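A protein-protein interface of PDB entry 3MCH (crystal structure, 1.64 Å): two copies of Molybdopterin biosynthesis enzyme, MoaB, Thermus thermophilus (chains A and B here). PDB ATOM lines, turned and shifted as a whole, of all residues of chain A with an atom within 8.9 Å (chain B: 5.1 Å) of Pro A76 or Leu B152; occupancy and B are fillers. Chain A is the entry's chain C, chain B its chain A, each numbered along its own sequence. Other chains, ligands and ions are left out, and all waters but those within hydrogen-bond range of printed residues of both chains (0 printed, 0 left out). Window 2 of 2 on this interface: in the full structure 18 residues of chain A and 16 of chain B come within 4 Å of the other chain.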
ATOM      1  N   ASP A  11     -14.588  13.560  -7.173  1.00  0.00           N
ATOM      2  CA  ASP A  11     -15.992  13.213  -7.379  1.00  0.00           C
ATOM      3  C   ASP A  11     -16.654  13.310  -6.008  1.00  0.00           C
ATOM      4  O   ASP A  11     -17.691  13.954  -5.855  1.00  0.00           O
ATOM      5  CB  ASP A  11     -16.155  11.776  -7.889  1.00  0.00           C
ATOM      6  CG  ASP A  11     -16.057  11.665  -9.400  1.00  0.00           C
ATOM      7  OD1 ASP A  11     -16.360  12.651 -10.106  1.00  0.00           O
ATOM      8  OD2 ASP A  11     -15.696  10.571  -9.880  1.00  0.00           O
ATOM      9  N   ASP A  45     -14.486  14.513 -11.041  1.00  0.00           N
ATOM     10  CA  ASP A  45     -13.513  13.914 -11.947  1.00  0.00           C
ATOM     11  C   ASP A  45     -14.068  13.864 -13.369  1.00  0.00           C
ATOM     12  O   ASP A  45     -14.277  12.787 -13.930  1.00  0.00           O
ATOM     13  CB  ASP A  45     -13.156  12.506 -11.465  1.00  0.00           C
ATOM     14  CG  ASP A  45     -12.336  12.520 -10.190  1.00  0.00           C
ATOM     15  OD1 ASP A  45     -11.164  12.950 -10.249  1.00  0.00           O
ATOM     16  OD2 ASP A  45     -12.857  12.108  -9.131  1.00  0.00           O
ATOM     17  N   PRO A  47     -13.257  15.609 -17.122  1.00  0.00           N
ATOM     18  CA  PRO A  47     -12.407  16.445 -17.975  1.00  0.00           C
ATOM     19  C   PRO A  47     -13.053  17.746 -18.455  1.00  0.00           C
ATOM     20  O   PRO A  47     -12.434  18.806 -18.395  1.00  0.00           O
ATOM     21  CB  PRO A  47     -12.049  15.506 -19.125  1.00  0.00           C
ATOM     22  CG  PRO A  47     -11.938  14.188 -18.426  1.00  0.00           C
ATOM     23  CD  PRO A  47     -13.160  14.193 -17.521  1.00  0.00           C
ATOM     24  N   GLY A  71      -7.401  13.547  -8.753  1.00  0.00           N
ATOM     25  CA  GLY A  71      -7.648  13.016 -10.080  1.00  0.00           C
ATOM     26  C   GLY A  71      -6.397  12.588 -10.822  1.00  0.00           C
ATOM     27  O   GLY A  71      -6.391  12.530 -12.053  1.00  0.00           O
ATOM     28  N   THR A  72      -5.331  12.275 -10.094  1.00  0.00           N
ATOM     29  CA  THR A  72      -4.098  11.863 -10.760  1.00  0.00           C
ATOM     30  C   THR A  72      -3.729  10.420 -10.456  1.00  0.00           C
ATOM     31  O   THR A  72      -2.664   9.949 -10.856  1.00  0.00           O
ATOM     32  CB  THR A  72      -2.913  12.773 -10.366  1.00  0.00           C
ATOM     33  OG1 THR A  72      -2.615  12.603  -8.975  1.00  0.00           O
ATOM     34  CG2 THR A  72      -3.256  14.230 -10.633  1.00  0.00           C
ATOM     35  N   GLY A  73      -4.624   9.722  -9.762  1.00  0.00           N
ATOM     36  CA  GLY A  73      -4.381   8.339  -9.404  1.00  0.00           C
ATOM     37  C   GLY A  73      -4.635   7.338 -10.515  1.00  0.00           C
ATOM     38  O   GLY A  73      -4.897   7.708 -11.661  1.00  0.00           O
ATOM     39  N   LEU A  74      -4.552   6.056 -10.164  1.00  0.00           N
ATOM     40  CA  LEU A  74      -4.756   4.970 -11.115  1.00  0.00           C
ATOM     41  C   LEU A  74      -6.208   4.525 -11.197  1.00  0.00           C
ATOM     42  O   LEU A  74      -6.524   3.550 -11.875  1.00  0.00           O
ATOM     43  CB  LEU A  74      -3.865   3.777 -10.745  1.00  0.00           C
ATOM     44  CG  LEU A  74      -2.424   3.794 -11.274  1.00  0.00           C
ATOM     45  CD1 LEU A  74      -1.780   5.141 -11.026  1.00  0.00           C
ATOM     46  CD2 LEU A  74      -1.618   2.678 -10.611  1.00  0.00           C
ATOM     47  N   ALA A  75      -7.090   5.232 -10.496  1.00  0.00           N
ATOM     48  CA  ALA A  75      -8.508   4.909 -10.537  1.00  0.00           C
ATOM     49  C   ALA A  75      -8.986   5.278 -11.937  1.00  0.00           C
ATOM     50  O   ALA A  75      -8.610   6.318 -12.475  1.00  0.00           O
ATOM     51  CB  ALA A  75      -9.269   5.708  -9.488  1.00  0.00           C
ATOM     52  N   PRO A  76      -9.822   4.426 -12.547  1.00  0.00           N
ATOM     53  CA  PRO A  76     -10.358   4.647 -13.894  1.00  0.00           C
ATOM     54  C   PRO A  76     -10.854   6.067 -14.176  1.00  0.00           C
ATOM     55  O   PRO A  76     -10.613   6.606 -15.257  1.00  0.00           O
ATOM     56  CB  PRO A  76     -11.479   3.616 -13.985  1.00  0.00           C
ATOM     57  CG  PRO A  76     -10.938   2.481 -13.184  1.00  0.00           C
ATOM     58  CD  PRO A  76     -10.364   3.182 -11.968  1.00  0.00           C
ATOM     59  N   ARG A  77     -11.542   6.673 -13.210  1.00  0.00           N
ATOM     60  CA  ARG A  77     -12.072   8.023 -13.395  1.00  0.00           C
ATOM     61  C   ARG A  77     -11.085   9.167 -13.171  1.00  0.00           C
ATOM     62  O   ARG A  77     -11.341  10.296 -13.591  1.00  0.00           O
ATOM     63  CB  ARG A  77     -13.316   8.228 -12.524  1.00  0.00           C
ATOM     64  CG  ARG A  77     -14.574   7.576 -13.100  1.00  0.00           C
ATOM     65  CD  ARG A  77     -15.794   7.871 -12.244  1.00  0.00           C
ATOM     66  NE  ARG A  77     -16.071   9.301 -12.162  1.00  0.00           N
ATOM     67  CZ  ARG A  77     -16.626  10.022 -13.133  1.00  0.00           C
ATOM     68  NH1 ARG A  77     -16.977   9.449 -14.279  1.00  0.00           N
ATOM     69  NH2 ARG A  77     -16.827  11.321 -12.958  1.00  0.00           N
ATOM     70  N   ASP A  78      -9.963   8.891 -12.515  1.00  0.00           N
ATOM     71  CA  ASP A  78      -8.953   9.930 -12.298  1.00  0.00           C
ATOM     72  C   ASP A  78      -8.412  10.335 -13.671  1.00  0.00           C
ATOM     73  O   ASP A  78      -7.625   9.603 -14.276  1.00  0.00           O
ATOM     74  CB  ASP A  78      -7.823   9.392 -11.413  1.00  0.00           C
ATOM     75  CG  ASP A  78      -8.166   9.436  -9.933  1.00  0.00           C
ATOM     76  OD1 ASP A  78      -9.367   9.457  -9.598  1.00  0.00           O
ATOM     77  OD2 ASP A  78      -7.235   9.444  -9.099  1.00  0.00           O
ATOM     78  N   ARG A  79      -8.830  11.500 -14.159  1.00  0.00           N
ATOM     79  CA  ARG A  79      -8.411  11.955 -15.480  1.00  0.00           C
ATOM     80  C   ARG A  79      -7.881  13.388 -15.552  1.00  0.00           C
ATOM     81  O   ARG A  79      -7.907  14.015 -16.612  1.00  0.00           O
ATOM     82  CB  ARG A  79      -9.577  11.785 -16.461  1.00  0.00           C
ATOM     83  CG  ARG A  79     -10.000  10.328 -16.644  1.00  0.00           C
ATOM     84  CD  ARG A  79     -11.350  10.220 -17.334  1.00  0.00           C
ATOM     85  NE  ARG A  79     -12.441  10.626 -16.453  1.00  0.00           N
ATOM     86  CZ  ARG A  79     -13.718  10.666 -16.819  1.00  0.00           C
ATOM     87  NH1 ARG A  79     -14.068  10.327 -18.052  1.00  0.00           N
ATOM     88  NH2 ARG A  79     -14.649  11.034 -15.950  1.00  0.00           N
ATOM     89  N   THR A  80      -7.384  13.904 -14.436  1.00  0.00           N
ATOM     90  CA  THR A  80      -6.849  15.259 -14.423  1.00  0.00           C
ATOM     91  C   THR A  80      -5.648  15.422 -15.356  1.00  0.00           C
ATOM     92  O   THR A  80      -5.522  16.438 -16.036  1.00  0.00           O
ATOM     93  CB  THR A  80      -6.448  15.669 -13.000  1.00  0.00           C
ATOM     94  OG1 THR A  80      -7.596  15.571 -12.148  1.00  0.00           O
ATOM     95  CG2 THR A  80      -5.931  17.108 -12.976  1.00  0.00           C
ATOM     96  N   GLU A  82      -4.886  13.793 -18.201  1.00  0.00           N
ATOM     97  CA  GLU A  82      -5.348  13.800 -19.586  1.00  0.00           C
ATOM     98  C   GLU A  82      -6.030  15.118 -19.925  1.00  0.00           C
ATOM     99  O   GLU A  82      -5.798  15.692 -20.989  1.00  0.00           O
ATOM    100  CB  GLU A  82      -6.326  12.643 -19.836  1.00  0.00           C
ATOM    101  CG  GLU A  82      -5.730  11.249 -19.669  1.00  0.00           C
ATOM    102  CD  GLU A  82      -5.936  10.668 -18.277  1.00  0.00           C
ATOM    103  OE1 GLU A  82      -5.513  11.299 -17.288  1.00  0.00           O
ATOM    104  OE2 GLU A  82      -6.523   9.569 -18.173  1.00  0.00           O
ATOM    105  N   MET A 109       4.623   6.448  -2.336  1.00  0.00           N
ATOM    106  CA  MET A 109       3.325   6.243  -2.958  1.00  0.00           C
ATOM    107  C   MET A 109       3.129   7.353  -3.987  1.00  0.00           C
ATOM    108  O   MET A 109       2.295   7.245  -4.885  1.00  0.00           O
ATOM    109  CB  MET A 109       2.214   6.318  -1.910  1.00  0.00           C
ATOM    110  CG  MET A 109       1.974   5.033  -1.138  1.00  0.00           C
ATOM    111  SD  MET A 109       1.286   3.724  -2.171  1.00  0.00           S
ATOM    112  CE  MET A 109       1.925   2.273  -1.324  1.00  0.00           C
ATOM    113  N   LEU A 112       2.856   6.918  -7.765  1.00  0.00           N
ATOM    114  CA  LEU A 112       1.632   6.515  -8.443  1.00  0.00           C
ATOM    115  C   LEU A 112       0.842   7.686  -9.016  1.00  0.00           C
ATOM    116  O   LEU A 112      -0.184   7.485  -9.662  1.00  0.00           O
ATOM    117  CB  LEU A 112       0.747   5.696  -7.501  1.00  0.00           C
ATOM    118  CG  LEU A 112       1.339   4.357  -7.049  1.00  0.00           C
ATOM    119  CD1 LEU A 112       0.290   3.592  -6.261  1.00  0.00           C
ATOM    120  CD2 LEU A 112       1.792   3.544  -8.254  1.00  0.00           C
ATOM    121  N   SER A 113       1.311   8.908  -8.788  1.00  0.00           N
ATOM    122  CA  SER A 113       0.615  10.071  -9.337  1.00  0.00           C
ATOM    123  C   SER A 113       1.009  10.264 -10.798  1.00  0.00           C
ATOM    124  O   SER A 113       2.193  10.274 -11.136  1.00  0.00           O
ATOM    125  CB  SER A 113       0.962  11.340  -8.557  1.00  0.00           C
ATOM    126  OG  SER A 113       0.347  12.473  -9.158  1.00  0.00           O
ATOM    127  N   ARG A 114       0.007  10.416 -11.661  1.00  0.00           N
ATOM    128  CA  ARG A 114       0.242  10.616 -13.082  1.00  0.00           C
ATOM    129  C   ARG A 114       0.190  12.100 -13.439  1.00  0.00           C
ATOM    130  O   ARG A 114       0.137  12.463 -14.607  1.00  0.00           O
ATOM    131  CB  ARG A 114      -0.806   9.858 -13.900  1.00  0.00           C
ATOM    132  CG  ARG A 114      -0.761   8.351 -13.728  1.00  0.00           C
ATOM    133  CD  ARG A 114      -1.927   7.694 -14.456  1.00  0.00           C
ATOM    134  NE  ARG A 114      -3.189   8.205 -13.938  1.00  0.00           N
ATOM    135  CZ  ARG A 114      -4.013   9.001 -14.612  1.00  0.00           C
ATOM    136  NH1 ARG A 114      -3.721   9.375 -15.851  1.00  0.00           N
ATOM    137  NH2 ARG A 114      -5.113   9.455 -14.025  1.00  0.00           N
ATOM    138  N   ARG B  90      -3.518   4.132 -20.808  1.00  0.00           N
ATOM    139  CA  ARG B  90      -2.840   5.235 -20.129  1.00  0.00           C
ATOM    140  C   ARG B  90      -1.525   4.743 -19.537  1.00  0.00           C
ATOM    141  O   ARG B  90      -1.363   3.555 -19.245  1.00  0.00           O
ATOM    142  CB  ARG B  90      -3.710   5.796 -19.000  1.00  0.00           C
ATOM    143  CG  ARG B  90      -4.090   4.757 -17.959  1.00  0.00           C
ATOM    144  CD  ARG B  90      -4.633   5.372 -16.677  1.00  0.00           C
ATOM    145  NE  ARG B  90      -5.747   6.282 -16.911  1.00  0.00           N
ATOM    146  CZ  ARG B  90      -6.505   6.797 -15.946  1.00  0.00           C
ATOM    147  NH1 ARG B  90      -6.270   6.489 -14.676  1.00  0.00           N
ATOM    148  NH2 ARG B  90      -7.496   7.623 -16.250  1.00  0.00           N
ATOM    149  N   ARG B 122      -8.234  -3.561 -17.364  1.00  0.00           N
ATOM    150  CA  ARG B 122      -8.042  -3.645 -15.919  1.00  0.00           C
ATOM    151  C   ARG B 122      -6.746  -4.401 -15.614  1.00  0.00           C
ATOM    152  O   ARG B 122      -6.631  -5.084 -14.595  1.00  0.00           O
ATOM    153  CB  ARG B 122      -9.238  -4.342 -15.256  1.00  0.00           C
ATOM    154  CG  ARG B 122     -10.572  -3.655 -15.521  1.00  0.00           C
ATOM    155  CD  ARG B 122     -11.619  -4.048 -14.492  1.00  0.00           C
ATOM    156  NE  ARG B 122     -11.429  -3.334 -13.232  1.00  0.00           N
ATOM    157  CZ  ARG B 122     -11.684  -2.039 -13.062  1.00  0.00           C
ATOM    158  NH1 ARG B 122     -11.475  -1.468 -11.883  1.00  0.00           N
ATOM    159  NH2 ARG B 122     -12.160  -1.317 -14.069  1.00  0.00           N
ATOM    160  N   HIS B 148      -1.014  -1.759  -3.925  1.00  0.00           N
ATOM    161  CA  HIS B 148      -1.927  -0.620  -3.920  1.00  0.00           C
ATOM    162  C   HIS B 148      -2.319  -0.229  -5.342  1.00  0.00           C
ATOM    163  O   HIS B 148      -3.493   0.002  -5.628  1.00  0.00           O
ATOM    164  CB  HIS B 148      -1.308   0.591  -3.218  1.00  0.00           C
ATOM    165  CG  HIS B 148      -2.252   1.745  -3.094  1.00  0.00           C
ATOM    166  ND1 HIS B 148      -3.454   1.653  -2.422  1.00  0.00           N
ATOM    167  CD2 HIS B 148      -2.195   3.005  -3.589  1.00  0.00           C
ATOM    168  CE1 HIS B 148      -4.096   2.804  -2.512  1.00  0.00           C
ATOM    169  NE2 HIS B 148      -3.355   3.641  -3.214  1.00  0.00           N
ATOM    170  N   ALA B 149      -1.331  -0.153  -6.225  1.00  0.00           N
ATOM    171  CA  ALA B 149      -1.578   0.199  -7.615  1.00  0.00           C
ATOM    172  C   ALA B 149      -2.559  -0.779  -8.258  1.00  0.00           C
ATOM    173  O   ALA B 149      -3.480  -0.373  -8.969  1.00  0.00           O
ATOM    174  CB  ALA B 149      -0.265   0.205  -8.394  1.00  0.00           C
ATOM    175  N   LEU B 150      -2.361  -2.070  -8.009  1.00  0.00           N
ATOM    176  CA  LEU B 150      -3.237  -3.087  -8.587  1.00  0.00           C
ATOM    177  C   LEU B 150      -4.661  -3.005  -8.051  1.00  0.00           C
ATOM    178  O   LEU B 150      -5.623  -3.224  -8.791  1.00  0.00           O
ATOM    179  CB  LEU B 150      -2.650  -4.484  -8.350  1.00  0.00           C
ATOM    180  CG  LEU B 150      -1.426  -4.792  -9.223  1.00  0.00           C
ATOM    181  CD1 LEU B 150      -0.678  -5.993  -8.678  1.00  0.00           C
ATOM    182  CD2 LEU B 150      -1.879  -5.037 -10.669  1.00  0.00           C
ATOM    183  N   SER B 151      -4.808  -2.680  -6.773  1.00  0.00           N
ATOM    184  CA  SER B 151      -6.149  -2.575  -6.212  1.00  0.00           C
ATOM    185  C   SER B 151      -6.928  -1.472  -6.930  1.00  0.00           C
ATOM    186  O   SER B 151      -8.124  -1.613  -7.185  1.00  0.00           O
ATOM    187  CB  SER B 151      -6.085  -2.305  -4.701  1.00  0.00           C
ATOM    188  OG  SER B 151      -5.496  -1.054  -4.410  1.00  0.00           O
ATOM    189  N   LEU B 152      -6.247  -0.381  -7.269  1.00  0.00           N
ATOM    190  CA  LEU B 152      -6.889   0.732  -7.964  1.00  0.00           C
ATOM    191  C   LEU B 152      -7.212   0.372  -9.412  1.00  0.00           C
ATOM    192  O   LEU B 152      -8.303   0.659  -9.909  1.00  0.00           O
ATOM    193  CB  LEU B 152      -5.982   1.965  -7.946  1.00  0.00           C
ATOM    194  CG  LEU B 152      -5.727   2.603  -6.580  1.00  0.00           C
ATOM    195  CD1 LEU B 152      -4.723   3.736  -6.713  1.00  0.00           C
ATOM    196  CD2 LEU B 152      -7.044   3.108  -6.008  1.00  0.00           C
ATOM    197  N   VAL B 153      -6.252  -0.258 -10.080  1.00  0.00           N
ATOM    198  CA  VAL B 153      -6.406  -0.650 -11.476  1.00  0.00           C
ATOM    199  C   VAL B 153      -7.442  -1.749 -11.692  1.00  0.00           C
ATOM    200  O   VAL B 153      -8.278  -1.656 -12.593  1.00  0.00           O
ATOM    201  CB  VAL B 153      -5.064  -1.143 -12.056  1.00  0.00           C
ATOM    202  CG1 VAL B 153      -5.268  -1.683 -13.475  1.00  0.00           C
ATOM    203  CG2 VAL B 153      -4.052  -0.008 -12.060  1.00  0.00           C
ATOM    204  N   THR B 154      -7.381  -2.783 -10.858  1.00  0.00           N
ATOM    205  CA  THR B 154      -8.271  -3.937 -10.973  1.00  0.00           C
ATOM    206  C   THR B 154      -9.600  -3.807 -10.241  1.00  0.00           C
ATOM    207  O   THR B 154     -10.572  -4.476 -10.596  1.00  0.00           O
ATOM    208  CB  THR B 154      -7.587  -5.209 -10.445  1.00  0.00           C
ATOM    209  OG1 THR B 154      -7.450  -5.115  -9.020  1.00  0.00           O
ATOM    210  CG2 THR B 154      -6.205  -5.379 -11.065  1.00  0.00           C
ATOM    211  N   GLY B 155      -9.638  -2.965  -9.214  1.00  0.00           N
ATOM    212  CA  GLY B 155     -10.860  -2.794  -8.446  1.00  0.00           C
ATOM    213  C   GLY B 155     -10.956  -3.830  -7.342  1.00  0.00           C
ATOM    214  O   GLY B 155     -11.881  -3.806  -6.528  1.00  0.00           O
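OE2 of Glu A82 lies within salt-bridge range of NH2 of Arg B90 (2.9 Å). The guanidinium group of Arg B90 sits close to the guanidinium group of Arg A114. The guanidinium group of Arg B90 lies within hydrogen-bond range of the backbone carbonyl oxygen of Ala A75 (3.2 Å). The guanidinium group (NH2) of Arg B90 is in hydrogen-bond range of the backbone carbonyl oxygen (O) of Asp A78 (2.8 Å). NH2 of Arg B90 is in hydrogen-bond range of O of Pro A76 (3.4 Å).
NH1 of Arg B122 lies within hydrogen-bond range of O of Val B153 (3.3 Å). OG of Ser B151 sits at hydrogen-bond distance from O of His B148, 2.6 Å away. The backbone NH (N) of Arg A114 lies within hydrogen-bond range of the backbone carbonyl oxygen (O) of Thr A72, 2.8 Å away. The backbone carbonyl oxygen (O) of Arg A77 lies within hydrogen-bond range of the guanidinium group (NE) of Arg A79. The backbone carbonyl oxygen (O) of Asp A78 is in hydrogen-bond range of the guanidinium group (NH2) of Arg A114 (2.5 Å). N of Gly A73 is in hydrogen-bond range of OD2 of Asp A78.
Of chain B, only Arg B90 and Leu B152 come within 4 Å of Pro A76. No residue of chain A comes within 4 Å of Ser B151. Printed residues of chain A within 4 Å of Val B153: Leu A74 (3.9 Å). Printed residues of chain B within 4 Å of Met A109: His B148. Asp A11 touches none of the printed residues of chain B. The nearest residue of chain B that does not touch Pro A76 is Arg B122 (4.1 Å).
No position is printed for both chains. Of the 15 pairs that touch across the chains among the printed residues, none has its exchanged pair printed and touching as well.
Hydrophobic or aromatic side chains of chain A that line the printed part of chain B: Leu A74, Pro A76, Met A109 and Leu A112. Among the printed residues, 15 pairs touch across the chains.
Gly A73 touches Arg B90. NH1 of Arg B90 touches C of Leu A74 (3.996 Å). Ala B149 touches Leu A74. Leu A74 touches Leu B152 (O to O, 3.9 Å). CD2 of Leu A74 touches CG2 of Val B153, 3.9 Å away. Pro A76 touches Leu B152. Arg A79 touches Arg B90. CD2 of His B148 touches SD of Met A109, at 3.8 Å. CD2 of His B148 touches CD1 of Leu A112 (3.7 Å). CB of Ala B149 touches CD2 of Leu A112, 3.9 Å away.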
